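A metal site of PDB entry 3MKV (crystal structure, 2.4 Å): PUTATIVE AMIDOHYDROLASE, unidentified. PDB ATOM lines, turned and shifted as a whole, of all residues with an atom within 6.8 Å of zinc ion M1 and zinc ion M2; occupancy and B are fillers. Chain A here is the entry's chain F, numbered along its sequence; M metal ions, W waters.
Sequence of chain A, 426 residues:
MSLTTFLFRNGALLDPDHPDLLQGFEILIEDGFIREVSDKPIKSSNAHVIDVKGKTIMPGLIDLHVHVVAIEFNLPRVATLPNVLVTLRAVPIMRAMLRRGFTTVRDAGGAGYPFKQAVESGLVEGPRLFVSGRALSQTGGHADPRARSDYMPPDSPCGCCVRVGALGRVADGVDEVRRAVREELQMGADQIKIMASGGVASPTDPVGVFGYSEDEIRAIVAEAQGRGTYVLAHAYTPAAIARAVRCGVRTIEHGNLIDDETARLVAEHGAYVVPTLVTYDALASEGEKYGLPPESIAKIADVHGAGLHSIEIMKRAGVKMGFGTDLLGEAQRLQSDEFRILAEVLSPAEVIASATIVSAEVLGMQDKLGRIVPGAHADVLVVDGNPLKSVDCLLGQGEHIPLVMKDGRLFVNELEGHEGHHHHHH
Asp 326 touches zinc ion M1 (OD2 to ZN, 2.9 Å). Of the 20 residues printed, 4 come within 4 Å of zinc ion M1.
Zinc ion M2 is bound by water W1 (2.1 Å), OQ1 of KCX 193 (2.1 Å), a ring nitrogen (NE2) of His 254 (2.3 Å) and a ring nitrogen (ND1) of His 234 (2.4 Å). Zinc ion M2 has four donor atoms within binding distance. Slightly farther from zinc ion M2 lies OQ2 of KCX 193 (2.8 Å).
Zinc ion M1 is bound by NE2 of His 65 (1.9 Å), NE2 of His 67 (2.1 Å) and OQ2 of KCX 193 (2.1 Å).
Residues that only touch zinc ion M2: Asp 326 (3.8 Å).
The side-chain carboxylate (OE1) of Glu 253 sits at hydrogen-bond distance from a ring nitrogen (ND1) of His 65, 2.4 Å away. The backbone carbonyl oxygen (O) of His 65 is in hydrogen-bond range of the backbone NH (N) of Asp 326, at 2.9 Å. NZ of KCX 193 sits close to the backbone carbonyl oxygen of Ala 108 (3.4 Å). A ring nitrogen (ND1) of His 67 is in hydrogen-bond range of the backbone carbonyl oxygen (O) of Gly 109 (3.2 Å). A ring nitrogen (ND1) of His 254 sits at hydrogen-bond distance from the side-chain hydroxyl (OG1) of Thr 276 (2.9 Å). The side-chain hydroxyl (OH) of Tyr 280 lies close to a ring nitrogen (ND1) of His 254, at 3.5 Å.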
ATOM      1  N   HIS A  65      16.670 -14.572  23.362  1.00  0.00           N
ATOM      2  CA  HIS A  65      16.105 -15.879  22.992  1.00  0.00           C
ATOM      3  C   HIS A  65      16.977 -17.098  23.353  1.00  0.00           C
ATOM      4  O   HIS A  65      17.732 -17.625  22.517  1.00  0.00           O
ATOM      5  CB  HIS A  65      15.761 -15.926  21.501  1.00  0.00           C
ATOM      6  CG  HIS A  65      14.903 -17.092  21.108  1.00  0.00           C
ATOM      7  ND1 HIS A  65      13.670 -16.942  20.513  1.00  0.00           N
ATOM      8  CD2 HIS A  65      15.105 -18.421  21.225  1.00  0.00           C
ATOM      9  CE1 HIS A  65      13.148 -18.132  20.277  1.00  0.00           C
ATOM     10  NE2 HIS A  65      14.000 -19.049  20.694  1.00  0.00           N
ATOM     11  N   VAL A  66      16.864 -17.542  24.601  1.00  0.00           N
ATOM     12  CA  VAL A  66      17.589 -18.724  25.048  1.00  0.00           C
ATOM     13  C   VAL A  66      16.628 -19.829  25.468  1.00  0.00           C
ATOM     14  O   VAL A  66      15.453 -19.581  25.747  1.00  0.00           O
ATOM     15  CB  VAL A  66      18.543 -18.415  26.227  1.00  0.00           C
ATOM     16  CG1 VAL A  66      19.751 -17.609  25.759  1.00  0.00           C
ATOM     17  CG2 VAL A  66      17.797 -17.681  27.341  1.00  0.00           C
ATOM     18  N   HIS A  67      17.140 -21.057  25.506  1.00  0.00           N
ATOM     19  CA  HIS A  67      16.401 -22.191  26.052  1.00  0.00           C
ATOM     20  C   HIS A  67      17.285 -22.911  27.074  1.00  0.00           C
ATOM     21  O   HIS A  67      17.959 -23.892  26.765  1.00  0.00           O
ATOM     22  CB  HIS A  67      15.926 -23.151  24.954  1.00  0.00           C
ATOM     23  CG  HIS A  67      14.901 -22.556  24.028  1.00  0.00           C
ATOM     24  ND1 HIS A  67      13.723 -22.009  24.476  1.00  0.00           N
ATOM     25  CD2 HIS A  67      14.889 -22.428  22.683  1.00  0.00           C
ATOM     26  CE1 HIS A  67      13.025 -21.559  23.456  1.00  0.00           C
ATOM     27  NE2 HIS A  67      13.709 -21.809  22.345  1.00  0.00           N
ATOM     28  N   ALA A 108      12.838 -18.457  26.138  1.00  0.00           N
ATOM     29  CA  ALA A 108      11.732 -18.522  25.193  1.00  0.00           C
ATOM     30  C   ALA A 108      10.881 -19.747  25.318  1.00  0.00           C
ATOM     31  O   ALA A 108      10.069 -20.029  24.467  1.00  0.00           O
ATOM     32  CB  ALA A 108      12.248 -18.361  23.784  1.00  0.00           C
ATOM     33  N   GLY A 109      11.073 -20.498  26.377  1.00  0.00           N
ATOM     34  CA  GLY A 109      10.273 -21.666  26.591  1.00  0.00           C
ATOM     35  C   GLY A 109      10.969 -22.787  27.290  1.00  0.00           C
ATOM     36  O   GLY A 109      11.978 -23.295  26.848  1.00  0.00           O
ATOM     37  N   HIS A 142       4.822 -26.422  16.261  1.00  0.00           N
ATOM     38  CA  HIS A 142       6.251 -26.453  16.565  1.00  0.00           C
ATOM     39  C   HIS A 142       6.560 -27.074  17.940  1.00  0.00           C
ATOM     40  O   HIS A 142       7.434 -27.940  18.043  1.00  0.00           O
ATOM     41  CB  HIS A 142       6.882 -25.058  16.406  1.00  0.00           C
ATOM     42  CG  HIS A 142       8.382 -25.074  16.406  1.00  0.00           C
ATOM     43  ND1 HIS A 142       9.118 -25.754  15.470  1.00  0.00           N
ATOM     44  CD2 HIS A 142       9.277 -24.487  17.242  1.00  0.00           C
ATOM     45  CE1 HIS A 142      10.403 -25.595  15.717  1.00  0.00           C
ATOM     46  NE2 HIS A 142      10.532 -24.834  16.791  1.00  0.00           N
ATOM     47  N   LEU A 167       9.627 -27.870  26.699  1.00  0.00           N
ATOM     48  CA  LEU A 167       9.756 -26.506  26.205  1.00  0.00           C
ATOM     49  C   LEU A 167       8.414 -25.837  25.892  1.00  0.00           C
ATOM     50  O   LEU A 167       8.298 -24.612  25.944  1.00  0.00           O
ATOM     51  CB  LEU A 167      10.701 -26.471  24.998  1.00  0.00           C
ATOM     52  CG  LEU A 167      12.178 -26.326  25.395  1.00  0.00           C
ATOM     53  CD1 LEU A 167      12.737 -27.619  26.015  1.00  0.00           C
ATOM     54  CD2 LEU A 167      13.024 -25.882  24.212  1.00  0.00           C
ATOM     55  N   KCX A 193       5.199 -16.898  25.276  1.00  0.00           N
ATOM     56  CA  KCX A 193       5.651 -17.442  23.992  1.00  0.00           C
ATOM     57  CB  KCX A 193       6.870 -18.340  24.188  1.00  0.00           C
ATOM     58  CG  KCX A 193       7.389 -19.012  22.900  1.00  0.00           C
ATOM     59  CD  KCX A 193       7.926 -17.951  21.928  1.00  0.00           C
ATOM     60  CE  KCX A 193       8.640 -18.546  20.724  1.00  0.00           C
ATOM     61  NZ  KCX A 193       9.672 -19.497  21.165  1.00  0.00           N
ATOM     62  C   KCX A 193       4.566 -18.289  23.304  1.00  0.00           C
ATOM     63  O   KCX A 193       3.877 -19.068  23.964  1.00  0.00           O
ATOM     64  CX  KCX A 193      10.595 -19.917  20.314  1.00  0.00           C
ATOM     65  OQ1 KCX A 193      10.595 -19.494  19.142  1.00  0.00           O
ATOM     66  OQ2 KCX A 193      11.458 -20.731  20.684  1.00  0.00           O
ATOM     67  N   MET A 195       3.999 -20.556  19.432  1.00  0.00           N
ATOM     68  CA  MET A 195       4.501 -20.897  18.099  1.00  0.00           C
ATOM     69  C   MET A 195       3.501 -20.443  17.040  1.00  0.00           C
ATOM     70  O   MET A 195       2.392 -20.999  16.934  1.00  0.00           O
ATOM     71  CB  MET A 195       4.818 -22.399  17.992  1.00  0.00           C
ATOM     72  CG  MET A 195       5.748 -22.908  19.082  1.00  0.00           C
ATOM     73  SD  MET A 195       7.367 -22.085  19.157  1.00  0.00           S
ATOM     74  CE  MET A 195       8.213 -23.044  20.416  1.00  0.00           C
ATOM     75  N   ALA A 233       6.414 -14.273  19.432  1.00  0.00           N
ATOM     76  CA  ALA A 233       5.974 -15.342  18.540  1.00  0.00           C
ATOM     77  C   ALA A 233       7.074 -15.869  17.627  1.00  0.00           C
ATOM     78  O   ALA A 233       7.798 -15.107  16.997  1.00  0.00           O
ATOM     79  CB  ALA A 233       4.802 -14.865  17.697  1.00  0.00           C
ATOM     80  N   HIS A 234       7.166 -17.193  17.531  1.00  0.00           N
ATOM     81  CA  HIS A 234       8.021 -17.863  16.562  1.00  0.00           C
ATOM     82  C   HIS A 234       7.381 -17.755  15.159  1.00  0.00           C
ATOM     83  O   HIS A 234       6.240 -18.163  14.975  1.00  0.00           O
ATOM     84  CB  HIS A 234       8.191 -19.321  16.986  1.00  0.00           C
ATOM     85  CG  HIS A 234       8.793 -20.211  15.937  1.00  0.00           C
ATOM     86  ND1 HIS A 234      10.091 -20.659  15.999  1.00  0.00           N
ATOM     87  CD2 HIS A 234       8.261 -20.746  14.816  1.00  0.00           C
ATOM     88  CE1 HIS A 234      10.334 -21.440  14.958  1.00  0.00           C
ATOM     89  NE2 HIS A 234       9.238 -21.503  14.220  1.00  0.00           N
ATOM     90  N   ALA A 235       8.098 -17.202  14.192  1.00  0.00           N
ATOM     91  CA  ALA A 235       7.550 -17.003  12.856  1.00  0.00           C
ATOM     92  C   ALA A 235       8.625 -16.720  11.795  1.00  0.00           C
ATOM     93  O   ALA A 235       9.503 -15.877  12.009  1.00  0.00           O
ATOM     94  CB  ALA A 235       6.503 -15.877  12.871  1.00  0.00           C
ATOM     95  N   TYR A 236       8.533 -17.400  10.656  1.00  0.00           N
ATOM     96  CA  TYR A 236       9.555 -17.272   9.601  1.00  0.00           C
ATOM     97  C   TYR A 236       9.083 -16.498   8.361  1.00  0.00           C
ATOM     98  O   TYR A 236       9.771 -15.596   7.875  1.00  0.00           O
ATOM     99  CB  TYR A 236      10.027 -18.648   9.155  1.00  0.00           C
ATOM    100  CG  TYR A 236      10.859 -19.414  10.157  1.00  0.00           C
ATOM    101  CD1 TYR A 236      12.127 -18.972  10.507  1.00  0.00           C
ATOM    102  CD2 TYR A 236      10.393 -20.592  10.726  1.00  0.00           C
ATOM    103  CE1 TYR A 236      12.904 -19.672  11.411  1.00  0.00           C
ATOM    104  CE2 TYR A 236      11.160 -21.302  11.628  1.00  0.00           C
ATOM    105  CZ  TYR A 236      12.427 -20.839  11.973  1.00  0.00           C
ATOM    106  OH  TYR A 236      13.203 -21.539  12.876  1.00  0.00           O
ATOM    107  N   GLU A 253      10.098 -13.840  16.727  1.00  0.00           N
ATOM    108  CA  GLU A 253      11.330 -14.614  16.854  1.00  0.00           C
ATOM    109  C   GLU A 253      11.848 -15.163  15.521  1.00  0.00           C
ATOM    110  O   GLU A 253      11.103 -15.774  14.764  1.00  0.00           O
ATOM    111  CB  GLU A 253      11.148 -15.767  17.857  1.00  0.00           C
ATOM    112  CG  GLU A 253      10.663 -15.330  19.225  1.00  0.00           C
ATOM    113  CD  GLU A 253      11.597 -14.322  19.903  1.00  0.00           C
ATOM    114  OE1 GLU A 253      12.733 -14.696  20.240  1.00  0.00           O
ATOM    115  OE2 GLU A 253      11.166 -13.165  20.114  1.00  0.00           O
ATOM    116  N   HIS A 254      13.136 -14.956  15.259  1.00  0.00           N
ATOM    117  CA  HIS A 254      13.770 -15.435  14.033  1.00  0.00           C
ATOM    118  C   HIS A 254      13.406 -14.582  12.833  1.00  0.00           C
ATOM    119  O   HIS A 254      14.220 -13.773  12.387  1.00  0.00           O
ATOM    120  CB  HIS A 254      13.433 -16.906  13.745  1.00  0.00           C
ATOM    121  CG  HIS A 254      13.274 -17.742  14.975  1.00  0.00           C
ATOM    122  ND1 HIS A 254      14.263 -17.889  15.922  1.00  0.00           N
ATOM    123  CD2 HIS A 254      12.233 -18.493  15.405  1.00  0.00           C
ATOM    124  CE1 HIS A 254      13.843 -18.679  16.884  1.00  0.00           C
ATOM    125  NE2 HIS A 254      12.608 -19.063  16.597  1.00  0.00           N
ATOM    126  N   THR A 276      17.953 -15.077  15.061  1.00  0.00           N
ATOM    127  CA  THR A 276      18.769 -16.005  15.806  1.00  0.00           C
ATOM    128  C   THR A 276      19.623 -16.814  14.857  1.00  0.00           C
ATOM    129  O   THR A 276      19.635 -18.042  14.892  1.00  0.00           O
ATOM    130  CB  THR A 276      17.909 -16.963  16.651  1.00  0.00           C
ATOM    131  OG1 THR A 276      17.198 -17.851  15.786  1.00  0.00           O
ATOM    132  CG2 THR A 276      16.930 -16.182  17.515  1.00  0.00           C
ATOM    133  N   TYR A 280      21.264 -21.746  13.194  1.00  0.00           N
ATOM    134  CA  TYR A 280      21.115 -22.473  11.940  1.00  0.00           C
ATOM    135  C   TYR A 280      22.456 -22.990  11.437  1.00  0.00           C
ATOM    136  O   TYR A 280      22.502 -23.979  10.706  1.00  0.00           O
ATOM    137  CB  TYR A 280      20.397 -21.595  10.903  1.00  0.00           C
ATOM    138  CG  TYR A 280      19.124 -21.016  11.476  1.00  0.00           C
ATOM    139  CD1 TYR A 280      17.957 -21.776  11.557  1.00  0.00           C
ATOM    140  CD2 TYR A 280      19.087 -19.709  11.955  1.00  0.00           C
ATOM    141  CE1 TYR A 280      16.803 -21.253  12.092  1.00  0.00           C
ATOM    142  CE2 TYR A 280      17.926 -19.180  12.495  1.00  0.00           C
ATOM    143  CZ  TYR A 280      16.779 -19.958  12.563  1.00  0.00           C
ATOM    144  OH  TYR A 280      15.628 -19.427  13.092  1.00  0.00           O
ATOM    145  N   ASP A 326      19.204 -18.749  20.330  1.00  0.00           N
ATOM    146  CA  ASP A 326      18.345 -19.955  20.226  1.00  0.00           C
ATOM    147  C   ASP A 326      19.142 -21.230  19.960  1.00  0.00           C
ATOM    148  O   ASP A 326      18.905 -21.921  18.967  1.00  0.00           O
ATOM    149  CB  ASP A 326      17.283 -19.759  19.131  1.00  0.00           C
ATOM    150  CG  ASP A 326      16.297 -20.919  19.062  1.00  0.00           C
ATOM    151  OD1 ASP A 326      16.384 -21.842  19.896  1.00  0.00           O
ATOM    152  OD2 ASP A 326      15.420 -20.913  18.172  1.00  0.00           O
ATOM    153  N   LEU A 327      20.064 -21.570  20.853  1.00  0.00           N
ATOM    154  CA  LEU A 327      20.937 -22.722  20.656  1.00  0.00           C
ATOM    155  C   LEU A 327      20.534 -23.921  21.518  1.00  0.00           C
ATOM    156  O   LEU A 327      19.973 -23.763  22.598  1.00  0.00           O
ATOM    157  CB  LEU A 327      22.383 -22.342  20.956  1.00  0.00           C
ATOM    158  CG  LEU A 327      23.014 -21.398  19.921  1.00  0.00           C
ATOM    159  CD1 LEU A 327      24.106 -20.573  20.581  1.00  0.00           C
ATOM    160  CD2 LEU A 327      23.543 -22.180  18.718  1.00  0.00           C
ATOM    161  N   LEU A 328      20.829 -25.116  21.020  1.00  0.00           N
ATOM    162  CA  LEU A 328      20.428 -26.349  21.689  1.00  0.00           C
ATOM    163  C   LEU A 328      21.626 -27.256  21.953  1.00  0.00           C
ATOM    164  O   LEU A 328      22.635 -27.205  21.255  1.00  0.00           O
ATOM    165  CB  LEU A 328      19.393 -27.088  20.856  1.00  0.00           C
ATOM    166  CG  LEU A 328      18.390 -26.208  20.110  1.00  0.00           C
ATOM    167  CD1 LEU A 328      17.677 -26.986  19.021  1.00  0.00           C
ATOM    168  CD2 LEU A 328      17.378 -25.555  21.065  1.00  0.00           C
HETATM  169 ZN    ZN M   1      13.583 -20.925  20.441  1.00  0.00          ZN
HETATM  170 ZN    ZN M   2      11.683 -20.803  17.854  1.00  0.00          ZN
HETATM  171  O   HOH W   1      11.587 -22.725  18.587  1.00  0.00           O
